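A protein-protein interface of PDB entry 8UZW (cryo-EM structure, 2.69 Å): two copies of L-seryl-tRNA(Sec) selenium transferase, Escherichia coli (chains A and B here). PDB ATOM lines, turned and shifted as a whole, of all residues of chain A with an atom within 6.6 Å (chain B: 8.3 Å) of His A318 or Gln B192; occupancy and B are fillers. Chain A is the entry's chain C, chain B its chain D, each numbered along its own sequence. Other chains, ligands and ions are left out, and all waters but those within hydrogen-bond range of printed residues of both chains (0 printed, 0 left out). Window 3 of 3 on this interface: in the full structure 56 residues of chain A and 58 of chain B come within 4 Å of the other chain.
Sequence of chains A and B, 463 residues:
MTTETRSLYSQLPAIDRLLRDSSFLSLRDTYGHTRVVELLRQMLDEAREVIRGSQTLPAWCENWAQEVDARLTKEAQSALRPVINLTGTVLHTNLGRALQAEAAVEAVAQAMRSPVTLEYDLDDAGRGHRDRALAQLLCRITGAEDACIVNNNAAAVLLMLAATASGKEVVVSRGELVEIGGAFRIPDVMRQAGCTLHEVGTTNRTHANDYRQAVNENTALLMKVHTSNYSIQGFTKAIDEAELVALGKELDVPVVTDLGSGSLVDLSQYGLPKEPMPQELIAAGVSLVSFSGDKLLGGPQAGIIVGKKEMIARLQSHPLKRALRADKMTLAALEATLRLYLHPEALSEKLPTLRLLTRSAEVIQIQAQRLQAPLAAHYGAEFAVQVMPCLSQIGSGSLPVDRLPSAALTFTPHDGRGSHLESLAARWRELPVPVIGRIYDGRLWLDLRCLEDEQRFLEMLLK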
ATOM      1  N   LEU A 158     -18.272  16.334 -14.598  1.00  0.00           N
ATOM      2  CA  LEU A 158     -17.006  15.619 -14.471  1.00  0.00           C
ATOM      3  C   LEU A 158     -16.117  16.248 -13.405  1.00  0.00           C
ATOM      4  O   LEU A 158     -15.578  15.549 -12.541  1.00  0.00           O
ATOM      5  CB  LEU A 158     -16.294  15.592 -15.821  1.00  0.00           C
ATOM      6  CG  LEU A 158     -14.843  15.126 -15.838  1.00  0.00           C
ATOM      7  CD1 LEU A 158     -14.767  13.650 -15.541  1.00  0.00           C
ATOM      8  CD2 LEU A 158     -14.223  15.438 -17.177  1.00  0.00           C
ATOM      9  N   LEU A 159     -15.949  17.573 -13.451  1.00  0.00           N
ATOM     10  CA  LEU A 159     -15.109  18.257 -12.472  1.00  0.00           C
ATOM     11  C   LEU A 159     -15.692  18.154 -11.071  1.00  0.00           C
ATOM     12  O   LEU A 159     -14.956  17.942 -10.102  1.00  0.00           O
ATOM     13  CB  LEU A 159     -14.933  19.722 -12.869  1.00  0.00           C
ATOM     14  CG  LEU A 159     -13.980  20.561 -12.021  1.00  0.00           C
ATOM     15  CD1 LEU A 159     -12.580  19.989 -12.060  1.00  0.00           C
ATOM     16  CD2 LEU A 159     -13.982  21.995 -12.500  1.00  0.00           C
ATOM     17  N   ALA A 162     -15.031  14.564  -9.875  1.00  0.00           N
ATOM     18  CA  ALA A 162     -13.614  14.280  -9.696  1.00  0.00           C
ATOM     19  C   ALA A 162     -12.998  15.079  -8.559  1.00  0.00           C
ATOM     20  O   ALA A 162     -12.008  14.634  -7.972  1.00  0.00           O
ATOM     21  CB  ALA A 162     -12.851  14.555 -10.992  1.00  0.00           C
ATOM     22  N   ALA A 163     -13.555  16.243  -8.231  1.00  0.00           N
ATOM     23  CA  ALA A 163     -13.001  17.078  -7.179  1.00  0.00           C
ATOM     24  C   ALA A 163     -13.649  16.854  -5.824  1.00  0.00           C
ATOM     25  O   ALA A 163     -12.994  17.074  -4.801  1.00  0.00           O
ATOM     26  CB  ALA A 163     -13.129  18.556  -7.555  1.00  0.00           C
ATOM     27  N   THR A 164     -14.908  16.421  -5.779  1.00  0.00           N
ATOM     28  CA  THR A 164     -15.585  16.234  -4.506  1.00  0.00           C
ATOM     29  C   THR A 164     -15.834  14.778  -4.142  1.00  0.00           C
ATOM     30  O   THR A 164     -16.138  14.498  -2.978  1.00  0.00           O
ATOM     31  CB  THR A 164     -16.922  16.988  -4.499  1.00  0.00           C
ATOM     32  OG1 THR A 164     -17.727  16.552  -5.599  1.00  0.00           O
ATOM     33  CG2 THR A 164     -16.686  18.483  -4.611  1.00  0.00           C
ATOM     34  N   SER A 166     -13.855  11.863  -5.652  1.00  0.00           N
ATOM     35  CA  SER A 166     -12.903  10.971  -6.297  1.00  0.00           C
ATOM     36  C   SER A 166     -12.551   9.813  -5.372  1.00  0.00           C
ATOM     37  O   SER A 166     -12.158  10.021  -4.221  1.00  0.00           O
ATOM     38  CB  SER A 166     -11.642  11.735  -6.694  1.00  0.00           C
ATOM     39  OG  SER A 166     -10.783  10.923  -7.472  1.00  0.00           O
ATOM     40  N   ALA A 313     -13.874  26.094  -4.117  1.00  0.00           N
ATOM     41  CA  ALA A 313     -12.423  26.174  -3.984  1.00  0.00           C
ATOM     42  C   ALA A 313     -11.770  24.830  -4.271  1.00  0.00           C
ATOM     43  O   ALA A 313     -10.681  24.772  -4.852  1.00  0.00           O
ATOM     44  CB  ALA A 313     -12.052  26.666  -2.588  1.00  0.00           C
ATOM     45  N   ARG A 314     -12.411  23.738  -3.851  1.00  0.00           N
ATOM     46  CA  ARG A 314     -11.928  22.411  -4.224  1.00  0.00           C
ATOM     47  C   ARG A 314     -11.980  22.214  -5.732  1.00  0.00           C
ATOM     48  O   ARG A 314     -11.086  21.597  -6.321  1.00  0.00           O
ATOM     49  CB  ARG A 314     -12.752  21.331  -3.526  1.00  0.00           C
ATOM     50  CG  ARG A 314     -12.513  21.223  -2.039  1.00  0.00           C
ATOM     51  CD  ARG A 314     -13.375  20.135  -1.429  1.00  0.00           C
ATOM     52  NE  ARG A 314     -12.849  18.805  -1.706  1.00  0.00           N
ATOM     53  CZ  ARG A 314     -13.406  17.679  -1.285  1.00  0.00           C
ATOM     54  NH1 ARG A 314     -14.520  17.685  -0.573  1.00  0.00           N
ATOM     55  NH2 ARG A 314     -12.830  16.518  -1.582  1.00  0.00           N
ATOM     56  N   LEU A 315     -13.036  22.717  -6.371  1.00  0.00           N
ATOM     57  CA  LEU A 315     -13.190  22.537  -7.812  1.00  0.00           C
ATOM     58  C   LEU A 315     -12.124  23.306  -8.586  1.00  0.00           C
ATOM     59  O   LEU A 315     -11.485  22.755  -9.491  1.00  0.00           O
ATOM     60  CB  LEU A 315     -14.591  22.972  -8.244  1.00  0.00           C
ATOM     61  CG  LEU A 315     -15.662  21.890  -8.385  1.00  0.00           C
ATOM     62  CD1 LEU A 315     -15.737  21.023  -7.149  1.00  0.00           C
ATOM     63  CD2 LEU A 315     -17.001  22.533  -8.648  1.00  0.00           C
ATOM     64  N   GLN A 316     -11.915  24.579  -8.243  1.00  0.00           N
ATOM     65  CA  GLN A 316     -10.962  25.407  -8.979  1.00  0.00           C
ATOM     66  C   GLN A 316      -9.527  24.940  -8.779  1.00  0.00           C
ATOM     67  O   GLN A 316      -8.663  25.225  -9.614  1.00  0.00           O
ATOM     68  CB  GLN A 316     -11.092  26.871  -8.560  1.00  0.00           C
ATOM     69  CG  GLN A 316     -12.511  27.403  -8.520  1.00  0.00           C
ATOM     70  CD  GLN A 316     -12.844  28.287  -9.701  1.00  0.00           C
ATOM     71  OE1 GLN A 316     -12.266  28.152 -10.776  1.00  0.00           O
ATOM     72  NE2 GLN A 316     -13.783  29.203  -9.505  1.00  0.00           N
ATOM     73  N   SER A 317      -9.251  24.242  -7.681  1.00  0.00           N
ATOM     74  CA  SER A 317      -7.908  23.758  -7.394  1.00  0.00           C
ATOM     75  C   SER A 317      -7.608  22.413  -8.040  1.00  0.00           C
ATOM     76  O   SER A 317      -6.461  21.960  -7.977  1.00  0.00           O
ATOM     77  CB  SER A 317      -7.708  23.652  -5.881  1.00  0.00           C
ATOM     78  OG  SER A 317      -8.428  24.667  -5.207  1.00  0.00           O
ATOM     79  N   HIS A 318      -8.597  21.769  -8.650  1.00  0.00           N
ATOM     80  CA  HIS A 318      -8.380  20.467  -9.252  1.00  0.00           C
ATOM     81  C   HIS A 318      -7.509  20.591 -10.500  1.00  0.00           C
ATOM     82  O   HIS A 318      -7.578  21.590 -11.217  1.00  0.00           O
ATOM     83  CB  HIS A 318      -9.711  19.816  -9.614  1.00  0.00           C
ATOM     84  CG  HIS A 318      -9.646  18.324  -9.711  1.00  0.00           C
ATOM     85  ND1 HIS A 318      -9.350  17.666 -10.884  1.00  0.00           N
ATOM     86  CD2 HIS A 318      -9.823  17.362  -8.775  1.00  0.00           C
ATOM     87  CE1 HIS A 318      -9.353  16.364 -10.670  1.00  0.00           C
ATOM     88  NE2 HIS A 318      -9.637  16.152  -9.398  1.00  0.00           N
ATOM     89  N   PRO A 319      -6.663  19.595 -10.764  1.00  0.00           N
ATOM     90  CA  PRO A 319      -5.868  19.626 -12.000  1.00  0.00           C
ATOM     91  C   PRO A 319      -6.709  19.625 -13.264  1.00  0.00           C
ATOM     92  O   PRO A 319      -6.256  20.135 -14.295  1.00  0.00           O
ATOM     93  CB  PRO A 319      -5.006  18.362 -11.891  1.00  0.00           C
ATOM     94  CG  PRO A 319      -4.958  18.054 -10.439  1.00  0.00           C
ATOM     95  CD  PRO A 319      -6.271  18.486  -9.878  1.00  0.00           C
ATOM     96  N   LEU A 320      -7.917  19.061 -13.221  1.00  0.00           N
ATOM     97  CA  LEU A 320      -8.785  19.047 -14.393  1.00  0.00           C
ATOM     98  C   LEU A 320      -9.228  20.439 -14.814  1.00  0.00           C
ATOM     99  O   LEU A 320      -9.544  20.639 -15.989  1.00  0.00           O
ATOM    100  CB  LEU A 320     -10.025  18.195 -14.131  1.00  0.00           C
ATOM    101  CG  LEU A 320     -10.060  16.756 -14.636  1.00  0.00           C
ATOM    102  CD1 LEU A 320     -11.328  16.086 -14.151  1.00  0.00           C
ATOM    103  CD2 LEU A 320      -9.981  16.720 -16.147  1.00  0.00           C
ATOM    104  N   LYS A 321      -9.255  21.398 -13.887  1.00  0.00           N
ATOM    105  CA  LYS A 321      -9.825  22.708 -14.183  1.00  0.00           C
ATOM    106  C   LYS A 321      -9.112  23.386 -15.343  1.00  0.00           C
ATOM    107  O   LYS A 321      -9.768  23.970 -16.210  1.00  0.00           O
ATOM    108  CB  LYS A 321      -9.778  23.585 -12.933  1.00  0.00           C
ATOM    109  CG  LYS A 321     -10.187  25.028 -13.155  1.00  0.00           C
ATOM    110  CD  LYS A 321     -11.646  25.146 -13.529  1.00  0.00           C
ATOM    111  CE  LYS A 321     -12.070  26.596 -13.600  1.00  0.00           C
ATOM    112  NZ  LYS A 321     -12.936  26.854 -14.776  1.00  0.00           N
ATOM    113  N   ARG A 322      -7.780  23.308 -15.387  1.00  0.00           N
ATOM    114  CA  ARG A 322      -7.045  23.850 -16.526  1.00  0.00           C
ATOM    115  C   ARG A 322      -7.534  23.270 -17.847  1.00  0.00           C
ATOM    116  O   ARG A 322      -7.666  23.997 -18.838  1.00  0.00           O
ATOM    117  CB  ARG A 322      -5.546  23.612 -16.362  1.00  0.00           C
ATOM    118  CG  ARG A 322      -4.759  24.273 -17.471  1.00  0.00           C
ATOM    119  CD  ARG A 322      -4.525  25.745 -17.274  1.00  0.00           C
ATOM    120  NE  ARG A 322      -3.470  26.223 -18.159  1.00  0.00           N
ATOM    121  CZ  ARG A 322      -3.600  26.338 -19.473  1.00  0.00           C
ATOM    122  NH1 ARG A 322      -4.719  26.002 -20.090  1.00  0.00           N
ATOM    123  NH2 ARG A 322      -2.583  26.805 -20.190  1.00  0.00           N
ATOM    124  N   VAL B 157      -3.751  17.797 -24.678  1.00  0.00           N
ATOM    125  CA  VAL B 157      -2.753  16.877 -24.138  1.00  0.00           C
ATOM    126  C   VAL B 157      -3.409  15.856 -23.218  1.00  0.00           C
ATOM    127  O   VAL B 157      -3.086  14.661 -23.262  1.00  0.00           O
ATOM    128  CB  VAL B 157      -1.642  17.659 -23.418  1.00  0.00           C
ATOM    129  CG1 VAL B 157      -0.616  16.710 -22.838  1.00  0.00           C
ATOM    130  CG2 VAL B 157      -0.981  18.619 -24.375  1.00  0.00           C
ATOM    131  N   LEU B 158      -4.340  16.305 -22.373  1.00  0.00           N
ATOM    132  CA  LEU B 158      -5.035  15.384 -21.480  1.00  0.00           C
ATOM    133  C   LEU B 158      -5.778  14.306 -22.261  1.00  0.00           C
ATOM    134  O   LEU B 158      -5.650  13.114 -21.965  1.00  0.00           O
ATOM    135  CB  LEU B 158      -6.001  16.160 -20.589  1.00  0.00           C
ATOM    136  CG  LEU B 158      -7.008  15.335 -19.797  1.00  0.00           C
ATOM    137  CD1 LEU B 158      -6.304  14.542 -18.726  1.00  0.00           C
ATOM    138  CD2 LEU B 158      -8.058  16.237 -19.198  1.00  0.00           C
ATOM    139  N   LEU B 161      -3.335  11.835 -24.075  1.00  0.00           N
ATOM    140  CA  LEU B 161      -2.690  10.856 -23.207  1.00  0.00           C
ATOM    141  C   LEU B 161      -3.697   9.878 -22.615  1.00  0.00           C
ATOM    142  O   LEU B 161      -3.373   8.705 -22.400  1.00  0.00           O
ATOM    143  CB  LEU B 161      -1.913  11.564 -22.101  1.00  0.00           C
ATOM    144  CG  LEU B 161      -0.657  12.325 -22.518  1.00  0.00           C
ATOM    145  CD1 LEU B 161      -0.124  13.125 -21.347  1.00  0.00           C
ATOM    146  CD2 LEU B 161       0.393  11.368 -23.046  1.00  0.00           C
ATOM    147  N   ALA B 162      -4.918  10.336 -22.332  1.00  0.00           N
ATOM    148  CA  ALA B 162      -5.918   9.450 -21.753  1.00  0.00           C
ATOM    149  C   ALA B 162      -6.521   8.503 -22.778  1.00  0.00           C
ATOM    150  O   ALA B 162      -7.025   7.442 -22.400  1.00  0.00           O
ATOM    151  CB  ALA B 162      -7.027  10.264 -21.088  1.00  0.00           C
ATOM    152  N   SER B 166      -3.515   5.398 -21.890  1.00  0.00           N
ATOM    153  CA  SER B 166      -4.065   5.218 -20.554  1.00  0.00           C
ATOM    154  C   SER B 166      -3.554   3.921 -19.941  1.00  0.00           C
ATOM    155  O   SER B 166      -3.669   2.850 -20.544  1.00  0.00           O
ATOM    156  CB  SER B 166      -5.591   5.218 -20.602  1.00  0.00           C
ATOM    157  OG  SER B 166      -6.137   5.202 -19.297  1.00  0.00           O
ATOM    158  N   ALA B 183      -0.335  26.574 -14.006  1.00  0.00           N
ATOM    159  CA  ALA B 183      -1.357  25.560 -13.798  1.00  0.00           C
ATOM    160  C   ALA B 183      -1.164  24.329 -14.671  1.00  0.00           C
ATOM    161  O   ALA B 183      -1.762  23.288 -14.383  1.00  0.00           O
ATOM    162  CB  ALA B 183      -2.749  26.145 -14.055  1.00  0.00           C
ATOM    163  N   ARG B 185       1.441  21.526 -15.974  1.00  0.00           N
ATOM    164  CA  ARG B 185       2.713  20.859 -15.739  1.00  0.00           C
ATOM    165  C   ARG B 185       2.646  19.492 -16.392  1.00  0.00           C
ATOM    166  O   ARG B 185       1.708  18.734 -16.135  1.00  0.00           O
ATOM    167  CB  ARG B 185       2.989  20.713 -14.243  1.00  0.00           C
ATOM    168  CG  ARG B 185       3.482  21.965 -13.554  1.00  0.00           C
ATOM    169  CD  ARG B 185       3.873  21.655 -12.122  1.00  0.00           C
ATOM    170  NE  ARG B 185       4.930  22.531 -11.635  1.00  0.00           N
ATOM    171  CZ  ARG B 185       5.591  22.345 -10.502  1.00  0.00           C
ATOM    172  NH1 ARG B 185       5.307  21.336  -9.695  1.00  0.00           N
ATOM    173  NH2 ARG B 185       6.564  23.188 -10.172  1.00  0.00           N
ATOM    174  N   ILE B 186       3.634  19.168 -17.228  1.00  0.00           N
ATOM    175  CA  ILE B 186       3.611  17.883 -17.931  1.00  0.00           C
ATOM    176  C   ILE B 186       3.530  16.699 -16.974  1.00  0.00           C
ATOM    177  O   ILE B 186       2.710  15.797 -17.216  1.00  0.00           O
ATOM    178  CB  ILE B 186       4.799  17.787 -18.904  1.00  0.00           C
ATOM    179  CG1 ILE B 186       4.507  18.592 -20.166  1.00  0.00           C
ATOM    180  CG2 ILE B 186       5.086  16.345 -19.270  1.00  0.00           C
ATOM    181  CD1 ILE B 186       3.338  18.070 -20.953  1.00  0.00           C
ATOM    182  N   PRO B 187       4.318  16.624 -15.894  1.00  0.00           N
ATOM    183  CA  PRO B 187       4.131  15.502 -14.959  1.00  0.00           C
ATOM    184  C   PRO B 187       2.729  15.423 -14.378  1.00  0.00           C
ATOM    185  O   PRO B 187       2.177  14.324 -14.244  1.00  0.00           O
ATOM    186  CB  PRO B 187       5.184  15.774 -13.878  1.00  0.00           C
ATOM    187  CG  PRO B 187       6.217  16.581 -14.558  1.00  0.00           C
ATOM    188  CD  PRO B 187       5.476  17.453 -15.510  1.00  0.00           C
ATOM    189  N   ASP B 188       2.117  16.566 -14.064  1.00  0.00           N
ATOM    190  CA  ASP B 188       0.797  16.553 -13.440  1.00  0.00           C
ATOM    191  C   ASP B 188      -0.298  16.197 -14.441  1.00  0.00           C
ATOM    192  O   ASP B 188      -1.234  15.462 -14.106  1.00  0.00           O
ATOM    193  CB  ASP B 188       0.523  17.904 -12.787  1.00  0.00           C
ATOM    194  CG  ASP B 188       1.554  18.257 -11.735  1.00  0.00           C
ATOM    195  OD1 ASP B 188       2.759  18.249 -12.057  1.00  0.00           O
ATOM    196  OD2 ASP B 188       1.162  18.535 -10.584  1.00  0.00           O
ATOM    197  N   VAL B 189      -0.205  16.709 -15.669  1.00  0.00           N
ATOM    198  CA  VAL B 189      -1.159  16.319 -16.705  1.00  0.00           C
ATOM    199  C   VAL B 189      -1.025  14.837 -17.017  1.00  0.00           C
ATOM    200  O   VAL B 189      -2.020  14.148 -17.269  1.00  0.00           O
ATOM    201  CB  VAL B 189      -0.969  17.181 -17.967  1.00  0.00           C
ATOM    202  CG1 VAL B 189      -2.047  16.868 -18.979  1.00  0.00           C
ATOM    203  CG2 VAL B 189      -1.023  18.643 -17.605  1.00  0.00           C
ATOM    204  N   MET B 190       0.204  14.327 -17.018  1.00  0.00           N
ATOM    205  CA  MET B 190       0.414  12.901 -17.227  1.00  0.00           C
ATOM    206  C   MET B 190      -0.171  12.074 -16.093  1.00  0.00           C
ATOM    207  O   MET B 190      -0.705  10.987 -16.333  1.00  0.00           O
ATOM    208  CB  MET B 190       1.904  12.623 -17.386  1.00  0.00           C
ATOM    209  CG  MET B 190       2.446  13.072 -18.720  1.00  0.00           C
ATOM    210  SD  MET B 190       3.948  12.202 -19.132  1.00  0.00           S
ATOM    211  CE  MET B 190       3.268  10.577 -19.385  1.00  0.00           C
ATOM    212  N   ARG B 191      -0.065  12.558 -14.856  1.00  0.00           N
ATOM    213  CA  ARG B 191      -0.689  11.857 -13.739  1.00  0.00           C
ATOM    214  C   ARG B 191      -2.207  11.857 -13.865  1.00  0.00           C
ATOM    215  O   ARG B 191      -2.855  10.837 -13.609  1.00  0.00           O
ATOM    216  CB  ARG B 191      -0.255  12.489 -12.420  1.00  0.00           C
ATOM    217  CG  ARG B 191      -0.395  11.576 -11.222  1.00  0.00           C
ATOM    218  CD  ARG B 191      -0.024  12.301  -9.944  1.00  0.00           C
ATOM    219  NE  ARG B 191       1.083  13.224 -10.158  1.00  0.00           N
ATOM    220  CZ  ARG B 191       2.362  12.874 -10.159  1.00  0.00           C
ATOM    221  NH1 ARG B 191       2.736  11.620  -9.963  1.00  0.00           N
ATOM    222  NH2 ARG B 191       3.288  13.805 -10.370  1.00  0.00           N
ATOM    223  N   GLN B 192      -2.793  12.992 -14.255  1.00  0.00           N
ATOM    224  CA  GLN B 192      -4.243  13.062 -14.419  1.00  0.00           C
ATOM    225  C   GLN B 192      -4.726  12.157 -15.542  1.00  0.00           C
ATOM    226  O   GLN B 192      -5.760  11.494 -15.415  1.00  0.00           O
ATOM    227  CB  GLN B 192      -4.681  14.500 -14.685  1.00  0.00           C
ATOM    228  CG  GLN B 192      -5.130  15.236 -13.450  1.00  0.00           C
ATOM    229  CD  GLN B 192      -6.342  14.602 -12.799  1.00  0.00           C
ATOM    230  OE1 GLN B 192      -7.326  14.282 -13.467  1.00  0.00           O
ATOM    231  NE2 GLN B 192      -6.275  14.412 -11.487  1.00  0.00           N
ATOM    232  N   ALA B 193      -3.994  12.120 -16.653  1.00  0.00           N
ATOM    233  CA  ALA B 193      -4.426  11.376 -17.827  1.00  0.00           C
ATOM    234  C   ALA B 193      -4.311   9.871 -17.658  1.00  0.00           C
ATOM    235  O   ALA B 193      -4.666   9.137 -18.585  1.00  0.00           O
ATOM    236  CB  ALA B 193      -3.625  11.823 -19.045  1.00  0.00           C
ATOM    237  N   GLY B 194      -3.827   9.389 -16.517  1.00  0.00           N
ATOM    238  CA  GLY B 194      -3.774   7.971 -16.251  1.00  0.00           C
ATOM    239  C   GLY B 194      -2.575   7.247 -16.813  1.00  0.00           C
ATOM    240  O   GLY B 194      -2.475   6.027 -16.636  1.00  0.00           O
ATOM    241  N   CYS B 195      -1.665   7.944 -17.482  1.00  0.00           N
ATOM    242  CA  CYS B 195      -0.459   7.318 -17.997  1.00  0.00           C
ATOM    243  C   CYS B 195       0.656   7.380 -16.960  1.00  0.00           C
ATOM    244  O   CYS B 195       0.540   8.025 -15.916  1.00  0.00           O
ATOM    245  CB  CYS B 195      -0.013   7.988 -19.296  1.00  0.00           C
ATOM    246  SG  CYS B 195      -0.330   9.754 -19.376  1.00  0.00           S
ATOM    247  N   LEU B 320     -13.880  11.361 -22.438  1.00  0.00           N
ATOM    248  CA  LEU B 320     -13.472  12.716 -22.084  1.00  0.00           C
ATOM    249  C   LEU B 320     -13.835  13.721 -23.166  1.00  0.00           C
ATOM    250  O   LEU B 320     -14.046  14.898 -22.862  1.00  0.00           O
ATOM    251  CB  LEU B 320     -11.967  12.767 -21.825  1.00  0.00           C
ATOM    252  CG  LEU B 320     -11.460  12.703 -20.387  1.00  0.00           C
ATOM    253  CD1 LEU B 320      -9.945  12.665 -20.383  1.00  0.00           C
ATOM    254  CD2 LEU B 320     -11.965  13.885 -19.590  1.00  0.00           C
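NE2 of His A318 is in hydrogen-bond range of O of Ala A162 (3.2 Å).
N of Leu A320 is in hydrogen-bond range of ND1 of His A318, 3.1 Å away.
Among the printed residues, pairs that only touch across the chains: Pro A319 with Gln B192 (3.5 Å), Leu A320 with Leu B158 (3.6 Å), Leu A158 with Leu B320 (3.7 Å), Arg A322 with Ala B183 (3.7 Å), His A318 with Gln B192 (3.7 Å) and Leu A320 with Gln B192 (3.9 Å).
Of chain B, only Gln B192 (3.7 Å) comes within 4 Å of His A318.
Of chain A, only His A318 (3.7 Å), Pro A319 (3.5 Å) and Leu A320 (3.9 Å) come within 4 Å of Gln B192.
Pro A319 touches one residue of chain B.
Printed residues of chain B within 4 Å of Leu A320: Leu B158 and Gln B192.
Of the printed residues of chain A, Ala B183 touches Arg A322.
Printed residues of chain B within 4 Å of Arg A322: Ala B183.
Of the printed residues of chain A, Leu B320 touches Leu A158.
Printed residues of chain B within 4 Å of Leu A158: Leu B320.
Ser B166 touches none of the printed residues of chain A.
The nearest residue of chain B that does not touch His A318 is Ala B183 (6.8 Å).
The nearest residue of chain A that does not touch Gln B192 is Ala A162 (6.1 Å).
The nearest printed residue of chain A that does not touch Leu B320 is Leu A320 (4.9 Å).
Hydrophobic or aromatic side chains of chain A that line the printed part of chain B: Leu A158, His A318, Pro A319 and Leu A320.
Leu A158 touches Leu B320, and with the chains exchanged Leu A320 touches Leu B158.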
